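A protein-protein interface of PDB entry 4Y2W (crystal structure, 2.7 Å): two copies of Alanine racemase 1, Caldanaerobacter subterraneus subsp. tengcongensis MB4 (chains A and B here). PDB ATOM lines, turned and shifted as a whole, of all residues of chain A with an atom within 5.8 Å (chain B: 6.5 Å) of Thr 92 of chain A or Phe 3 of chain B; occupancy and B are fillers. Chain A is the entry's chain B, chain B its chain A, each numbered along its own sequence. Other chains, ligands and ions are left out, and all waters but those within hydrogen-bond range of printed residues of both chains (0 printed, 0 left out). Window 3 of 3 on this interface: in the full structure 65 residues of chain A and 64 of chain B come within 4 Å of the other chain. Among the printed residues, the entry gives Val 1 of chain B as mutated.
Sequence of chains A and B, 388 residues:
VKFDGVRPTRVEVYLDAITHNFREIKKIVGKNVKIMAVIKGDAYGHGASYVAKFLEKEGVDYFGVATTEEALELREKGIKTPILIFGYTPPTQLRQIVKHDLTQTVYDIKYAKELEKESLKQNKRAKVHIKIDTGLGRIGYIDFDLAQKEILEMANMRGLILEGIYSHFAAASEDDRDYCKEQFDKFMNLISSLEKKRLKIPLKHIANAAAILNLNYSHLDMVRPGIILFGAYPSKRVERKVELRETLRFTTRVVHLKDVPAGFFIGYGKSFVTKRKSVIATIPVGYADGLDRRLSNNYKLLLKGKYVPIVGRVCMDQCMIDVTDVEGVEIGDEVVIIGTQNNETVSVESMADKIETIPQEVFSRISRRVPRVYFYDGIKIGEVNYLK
The backbone carbonyl oxygen (O) of Asp 4 of chain B is in hydrogen-bond range of the side-chain hydroxyl (OG1) of Thr 92 of chain A (3.1 Å). O of Asp 4 of chain B is in hydrogen-bond range of NE2 of Gln 93 of chain A. NE2 of Gln 93 of chain A sits at hydrogen-bond distance from O of Gly 5 of chain B (3.2 Å). O of Val 6 of chain B lies within hydrogen-bond range of NE2 of Gln 93 of chain A (3.4 Å).
OD1 of Asp 4 of chain B sits at hydrogen-bond distance from N of Val 6 of chain B (2.9 Å). The guanidinium group (NH2) of Arg 10 of chain B lies within salt-bridge range of the side-chain carboxylate (OD1) of Asp 4 of chain B, at 2.8 Å. The backbone carbonyl oxygen (O) of Val 6 of chain B sits at hydrogen-bond distance from the guanidinium group (NH2) of Arg 10 of chain B (3.1 Å).
Among the printed residues, pairs that only touch across the chains: Tyr 88 of chain A with Phe 3 of chain B (3.8 Å), Tyr 88 of chain A with Val 255 of chain B (3.5 Å), Pro 90 of chain A with Phe 3 of chain B (3.5 Å) and Thr 92 of chain A with Phe 3 of chain B (3.5 Å).
Printed residues of chain B within 4 Å of Pro 90 of chain A: Phe 3 (3.5 Å). Thr 92 of chain A touches just these residues of chain B: Phe 3 (3.5 Å) and Asp 4 (3.1 Å). Of chain A, only Tyr 88, Pro 90 and Thr 92 come within 4 Å of Phe 3 of chain B. Of the printed residues of chain A, Asp 4 of chain B touches Thr 92 and Gln 93. Printed residues of chain A within 4 Å of Val 6 of chain B: Gln 93 (3.4 Å). Pro 8 of chain B touches none of the printed residues of chain A. Of the printed residues of chain A, Val 255 of chain B touches Tyr 88. Gly 332 of chain B touches none of the printed residues of chain A. The nearest residue of chain B that does not touch Thr 92 of chain A is Gly 5 of chain B (4.4 Å). The nearest residue of chain A that does not touch Phe 3 of chain B is Pro 91 of chain A (4.2 Å). The nearest printed residue of chain A that does not touch Gly 5 of chain B is Thr 92 of chain A (4.4 Å).
Of the 14 printed residues of chain B, 5 touch a printed residue of chain A. Printed residues of chain B that touch a printed residue of chain A: Phe 3, Asp 4, Gly 5, Val 6 and Val 255. Hydrophobic or aromatic side chains of chain B that line the printed part of chain A: Phe 3 and Val 255. Of the 7 printed residues of chain A, 4 touch a printed residue of chain B. Among the printed residues, no Asp or Glu carboxylate lies within 4 Å of a Lys or Arg side-chain nitrogen of the other chain.
No position is printed for both chains. Of the 8 pairs that touch across the chains among the printed residues, none has its exchanged pair printed and touching as well.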
ATOM      1  N   TYR A  88      35.903  26.493  -3.865  1.00  0.00           N
ATOM      2  CA  TYR A  88      35.191  25.534  -3.036  1.00  0.00           C
ATOM      3  C   TYR A  88      35.047  24.203  -3.765  1.00  0.00           C
ATOM      4  O   TYR A  88      34.457  24.143  -4.843  1.00  0.00           O
ATOM      5  CB  TYR A  88      33.812  26.106  -2.699  1.00  0.00           C
ATOM      6  CG  TYR A  88      32.891  25.208  -1.890  1.00  0.00           C
ATOM      7  CD1 TYR A  88      33.090  25.013  -0.528  1.00  0.00           C
ATOM      8  CD2 TYR A  88      31.792  24.587  -2.486  1.00  0.00           C
ATOM      9  CE1 TYR A  88      32.236  24.207   0.212  1.00  0.00           C
ATOM     10  CE2 TYR A  88      30.932  23.785  -1.753  1.00  0.00           C
ATOM     11  CZ  TYR A  88      31.158  23.597  -0.408  1.00  0.00           C
ATOM     12  OH  TYR A  88      30.306  22.799   0.318  1.00  0.00           O
ATOM     13  N   PRO A  90      33.097  20.924  -3.732  1.00  0.00           N
ATOM     14  CA  PRO A  90      31.891  20.450  -3.053  1.00  0.00           C
ATOM     15  C   PRO A  90      32.069  19.083  -2.382  1.00  0.00           C
ATOM     16  O   PRO A  90      32.900  18.292  -2.828  1.00  0.00           O
ATOM     17  CB  PRO A  90      30.844  20.381  -4.175  1.00  0.00           C
ATOM     18  CG  PRO A  90      31.607  20.409  -5.449  1.00  0.00           C
ATOM     19  CD  PRO A  90      32.868  21.163  -5.168  1.00  0.00           C
ATOM     20  N   PRO A  91      31.291  18.809  -1.317  1.00  0.00           N
ATOM     21  CA  PRO A  91      31.325  17.543  -0.577  1.00  0.00           C
ATOM     22  C   PRO A  91      31.269  16.290  -1.452  1.00  0.00           C
ATOM     23  O   PRO A  91      31.778  15.243  -1.055  1.00  0.00           O
ATOM     24  CB  PRO A  91      30.068  17.617   0.289  1.00  0.00           C
ATOM     25  CG  PRO A  91      29.876  19.069   0.530  1.00  0.00           C
ATOM     26  CD  PRO A  91      30.322  19.753  -0.729  1.00  0.00           C
ATOM     27  N   THR A  92      30.646  16.404  -2.621  1.00  0.00           N
ATOM     28  CA  THR A  92      30.548  15.294  -3.560  1.00  0.00           C
ATOM     29  C   THR A  92      31.875  14.920  -4.218  1.00  0.00           C
ATOM     30  O   THR A  92      32.003  13.812  -4.730  1.00  0.00           O
ATOM     31  CB  THR A  92      29.516  15.598  -4.671  1.00  0.00           C
ATOM     32  OG1 THR A  92      29.732  16.917  -5.191  1.00  0.00           O
ATOM     33  CG2 THR A  92      28.101  15.505  -4.128  1.00  0.00           C
ATOM     34  N   GLN A  93      32.851  15.828  -4.214  1.00  0.00           N
ATOM     35  CA  GLN A  93      34.115  15.609  -4.928  1.00  0.00           C
ATOM     36  C   GLN A  93      35.350  15.623  -4.017  1.00  0.00           C
ATOM     37  O   GLN A  93      36.468  15.850  -4.486  1.00  0.00           O
ATOM     38  CB  GLN A  93      34.285  16.676  -6.016  1.00  0.00           C
ATOM     39  CG  GLN A  93      33.100  16.825  -6.956  1.00  0.00           C
ATOM     40  CD  GLN A  93      33.229  18.033  -7.866  1.00  0.00           C
ATOM     41  OE1 GLN A  93      34.338  18.462  -8.200  1.00  0.00           O
ATOM     42  NE2 GLN A  93      32.093  18.590  -8.272  1.00  0.00           N
ATOM     43  N   LEU A  94      35.160  15.368  -2.726  1.00  0.00           N
ATOM     44  CA  LEU A  94      36.267  15.405  -1.771  1.00  0.00           C
ATOM     45  C   LEU A  94      37.184  14.183  -1.873  1.00  0.00           C
ATOM     46  O   LEU A  94      38.341  14.245  -1.458  1.00  0.00           O
ATOM     47  CB  LEU A  94      35.743  15.549  -0.340  1.00  0.00           C
ATOM     48  CG  LEU A  94      35.007  16.852  -0.026  1.00  0.00           C
ATOM     49  CD1 LEU A  94      34.461  16.821   1.395  1.00  0.00           C
ATOM     50  CD2 LEU A  94      35.911  18.060  -0.229  1.00  0.00           C
ATOM     51  N   ARG A  95      36.674  13.078  -2.413  1.00  0.00           N
ATOM     52  CA  ARG A  95      37.494  11.884  -2.623  1.00  0.00           C
ATOM     53  C   ARG A  95      38.698  12.157  -3.537  1.00  0.00           C
ATOM     54  O   ARG A  95      39.792  11.647  -3.292  1.00  0.00           O
ATOM     55  CB  ARG A  95      36.649  10.743  -3.198  1.00  0.00           C
ATOM     56  CG  ARG A  95      37.435   9.459  -3.416  1.00  0.00           C
ATOM     57  CD  ARG A  95      36.619   8.363  -4.082  1.00  0.00           C
ATOM     58  NE  ARG A  95      37.491   7.473  -4.851  1.00  0.00           N
ATOM     59  CZ  ARG A  95      38.330   6.575  -4.326  1.00  0.00           C
ATOM     60  NH1 ARG A  95      38.432   6.409  -3.006  1.00  0.00           N
ATOM     61  NH2 ARG A  95      39.080   5.828  -5.131  1.00  0.00           N
ATOM     62  N   VAL B   1      19.776  18.038  -7.417  1.00  0.00           N
ATOM     63  CA  VAL B   1      20.539  18.016  -6.128  1.00  0.00           C
ATOM     64  C   VAL B   1      21.399  19.272  -5.985  1.00  0.00           C
ATOM     65  O   VAL B   1      21.600  20.008  -6.955  1.00  0.00           O
ATOM     66  CB  VAL B   1      21.437  16.755  -6.000  1.00  0.00           C
ATOM     67  CG1 VAL B   1      20.606  15.532  -5.625  1.00  0.00           C
ATOM     68  CG2 VAL B   1      22.225  16.504  -7.282  1.00  0.00           C
ATOM     69  N   LYS B   2      21.899  19.504  -4.770  1.00  0.00           N
ATOM     70  CA  LYS B   2      22.765  20.652  -4.480  1.00  0.00           C
ATOM     71  C   LYS B   2      24.073  20.570  -5.272  1.00  0.00           C
ATOM     72  O   LYS B   2      24.355  21.429  -6.113  1.00  0.00           O
ATOM     73  CB  LYS B   2      23.078  20.736  -2.980  1.00  0.00           C
ATOM     74  CG  LYS B   2      21.885  21.034  -2.080  1.00  0.00           C
ATOM     75  CD  LYS B   2      22.297  21.005  -0.611  1.00  0.00           C
ATOM     76  CE  LYS B   2      21.103  21.019   0.340  1.00  0.00           C
ATOM     77  NZ  LYS B   2      20.443  22.352   0.438  1.00  0.00           N
ATOM     78  N   PHE B   3      24.861  19.530  -5.006  1.00  0.00           N
ATOM     79  CA  PHE B   3      26.147  19.335  -5.671  1.00  0.00           C
ATOM     80  C   PHE B   3      26.249  17.935  -6.263  1.00  0.00           C
ATOM     81  O   PHE B   3      25.495  17.037  -5.891  1.00  0.00           O
ATOM     82  CB  PHE B   3      27.292  19.571  -4.688  1.00  0.00           C
ATOM     83  CG  PHE B   3      27.358  20.978  -4.166  1.00  0.00           C
ATOM     84  CD1 PHE B   3      27.749  22.020  -4.996  1.00  0.00           C
ATOM     85  CD2 PHE B   3      27.017  21.263  -2.852  1.00  0.00           C
ATOM     86  CE1 PHE B   3      27.808  23.322  -4.521  1.00  0.00           C
ATOM     87  CE2 PHE B   3      27.073  22.562  -2.371  1.00  0.00           C
ATOM     88  CZ  PHE B   3      27.472  23.592  -3.205  1.00  0.00           C
ATOM     89  N   ASP B   4      27.184  17.767  -7.192  1.00  0.00           N
ATOM     90  CA  ASP B   4      27.384  16.490  -7.878  1.00  0.00           C
ATOM     91  C   ASP B   4      28.782  16.445  -8.493  1.00  0.00           C
ATOM     92  O   ASP B   4      29.594  17.326  -8.238  1.00  0.00           O
ATOM     93  CB  ASP B   4      26.297  16.285  -8.946  1.00  0.00           C
ATOM     94  CG  ASP B   4      26.321  17.355 -10.028  1.00  0.00           C
ATOM     95  OD1 ASP B   4      27.336  18.069 -10.156  1.00  0.00           O
ATOM     96  OD2 ASP B   4      25.318  17.480 -10.757  1.00  0.00           O
ATOM     97  N   GLY B   5      29.058  15.425  -9.299  1.00  0.00           N
ATOM     98  CA  GLY B   5      30.361  15.272  -9.941  1.00  0.00           C
ATOM     99  C   GLY B   5      30.793  16.440 -10.809  1.00  0.00           C
ATOM    100  O   GLY B   5      31.983  16.718 -10.922  1.00  0.00           O
ATOM    101  N   VAL B   6      29.830  17.127 -11.418  1.00  0.00           N
ATOM    102  CA  VAL B   6      30.115  18.243 -12.320  1.00  0.00           C
ATOM    103  C   VAL B   6      30.341  19.531 -11.528  1.00  0.00           C
ATOM    104  O   VAL B   6      29.780  19.710 -10.447  1.00  0.00           O
ATOM    105  CB  VAL B   6      28.964  18.446 -13.332  1.00  0.00           C
ATOM    106  CG1 VAL B   6      29.250  19.617 -14.269  1.00  0.00           C
ATOM    107  CG2 VAL B   6      28.743  17.173 -14.137  1.00  0.00           C
ATOM    108  N   PRO B   8      30.078  23.175 -10.002  1.00  0.00           N
ATOM    109  CA  PRO B   8      28.864  23.926  -9.679  1.00  0.00           C
ATOM    110  C   PRO B   8      28.450  24.889 -10.795  1.00  0.00           C
ATOM    111  O   PRO B   8      27.311  24.830 -11.262  1.00  0.00           O
ATOM    112  CB  PRO B   8      29.249  24.681  -8.403  1.00  0.00           C
ATOM    113  CG  PRO B   8      30.311  23.850  -7.779  1.00  0.00           C
ATOM    114  CD  PRO B   8      31.081  23.272  -8.925  1.00  0.00           C
ATOM    115  N   ARG B  10      27.966  25.911 -14.353  1.00  0.00           N
ATOM    116  CA  ARG B  10      27.735  25.033 -15.503  1.00  0.00           C
ATOM    117  C   ARG B  10      26.769  25.609 -16.529  1.00  0.00           C
ATOM    118  O   ARG B  10      26.009  26.536 -16.243  1.00  0.00           O
ATOM    119  CB  ARG B  10      27.176  23.692 -15.026  1.00  0.00           C
ATOM    120  CG  ARG B  10      25.777  23.774 -14.425  1.00  0.00           C
ATOM    121  CD  ARG B  10      25.363  22.459 -13.791  1.00  0.00           C
ATOM    122  NE  ARG B  10      26.188  22.119 -12.632  1.00  0.00           N
ATOM    123  CZ  ARG B  10      26.111  20.973 -11.959  1.00  0.00           C
ATOM    124  NH1 ARG B  10      25.245  20.030 -12.311  1.00  0.00           N
ATOM    125  NH2 ARG B  10      26.911  20.767 -10.922  1.00  0.00           N
ATOM    126  N   ARG B 253      26.094  27.874  -8.263  1.00  0.00           N
ATOM    127  CA  ARG B 253      25.579  27.517  -6.940  1.00  0.00           C
ATOM    128  C   ARG B 253      26.054  28.460  -5.844  1.00  0.00           C
ATOM    129  O   ARG B 253      27.105  29.095  -5.959  1.00  0.00           O
ATOM    130  CB  ARG B 253      25.996  26.091  -6.578  1.00  0.00           C
ATOM    131  CG  ARG B 253      25.507  25.025  -7.543  1.00  0.00           C
ATOM    132  CD  ARG B 253      24.031  24.726  -7.359  1.00  0.00           C
ATOM    133  NE  ARG B 253      23.466  24.076  -8.541  1.00  0.00           N
ATOM    134  CZ  ARG B 253      22.337  23.368  -8.566  1.00  0.00           C
ATOM    135  NH1 ARG B 253      21.608  23.184  -7.464  1.00  0.00           N
ATOM    136  NH2 ARG B 253      21.938  22.827  -9.709  1.00  0.00           N
ATOM    137  N   VAL B 254      25.273  28.531  -4.768  1.00  0.00           N
ATOM    138  CA  VAL B 254      25.670  29.298  -3.599  1.00  0.00           C
ATOM    139  C   VAL B 254      26.760  28.507  -2.883  1.00  0.00           C
ATOM    140  O   VAL B 254      26.580  27.333  -2.547  1.00  0.00           O
ATOM    141  CB  VAL B 254      24.486  29.594  -2.654  1.00  0.00           C
ATOM    142  CG1 VAL B 254      24.959  30.387  -1.443  1.00  0.00           C
ATOM    143  CG2 VAL B 254      23.395  30.365  -3.389  1.00  0.00           C
ATOM    144  N   VAL B 255      27.894  29.165  -2.684  1.00  0.00           N
ATOM    145  CA  VAL B 255      29.099  28.541  -2.153  1.00  0.00           C
ATOM    146  C   VAL B 255      29.467  29.091  -0.768  1.00  0.00           C
ATOM    147  O   VAL B 255      30.197  28.445  -0.019  1.00  0.00           O
ATOM    148  CB  VAL B 255      30.250  28.701  -3.190  1.00  0.00           C
ATOM    149  CG1 VAL B 255      31.569  29.158  -2.572  1.00  0.00           C
ATOM    150  CG2 VAL B 255      30.421  27.419  -3.992  1.00  0.00           C
ATOM    151  N   ILE B 331      23.296  26.787   1.197  1.00  0.00           N
ATOM    152  CA  ILE B 331      24.483  26.426   0.435  1.00  0.00           C
ATOM    153  C   ILE B 331      24.063  25.396  -0.606  1.00  0.00           C
ATOM    154  O   ILE B 331      23.469  24.373  -0.263  1.00  0.00           O
ATOM    155  CB  ILE B 331      25.583  25.823   1.340  1.00  0.00           C
ATOM    156  CG1 ILE B 331      25.981  26.799   2.462  1.00  0.00           C
ATOM    157  CG2 ILE B 331      26.797  25.418   0.516  1.00  0.00           C
ATOM    158  CD1 ILE B 331      26.473  28.151   1.988  1.00  0.00           C
ATOM    159  N   GLY B 332      24.355  25.674  -1.874  1.00  0.00           N
ATOM    160  CA  GLY B 332      24.005  24.768  -2.963  1.00  0.00           C
ATOM    161  C   GLY B 332      22.682  25.074  -3.642  1.00  0.00           C
ATOM    162  O   GLY B 332      22.206  24.281  -4.458  1.00  0.00           O
ATOM    163  N   ASP B 333      22.075  26.212  -3.311  1.00  0.00           N
ATOM    164  CA  ASP B 333      20.919  26.686  -4.065  1.00  0.00           C
ATOM    165  C   ASP B 333      21.383  27.131  -5.446  1.00  0.00           C
ATOM    166  O   ASP B 333      22.446  27.737  -5.586  1.00  0.00           O
ATOM    167  CB  ASP B 333      20.212  27.841  -3.352  1.00  0.00           C
ATOM    168  CG  ASP B 333      19.421  27.386  -2.136  1.00  0.00           C
ATOM    169  OD1 ASP B 333      19.130  26.171  -2.016  1.00  0.00           O
ATOM    170  OD2 ASP B 333      19.087  28.252  -1.296  1.00  0.00           O
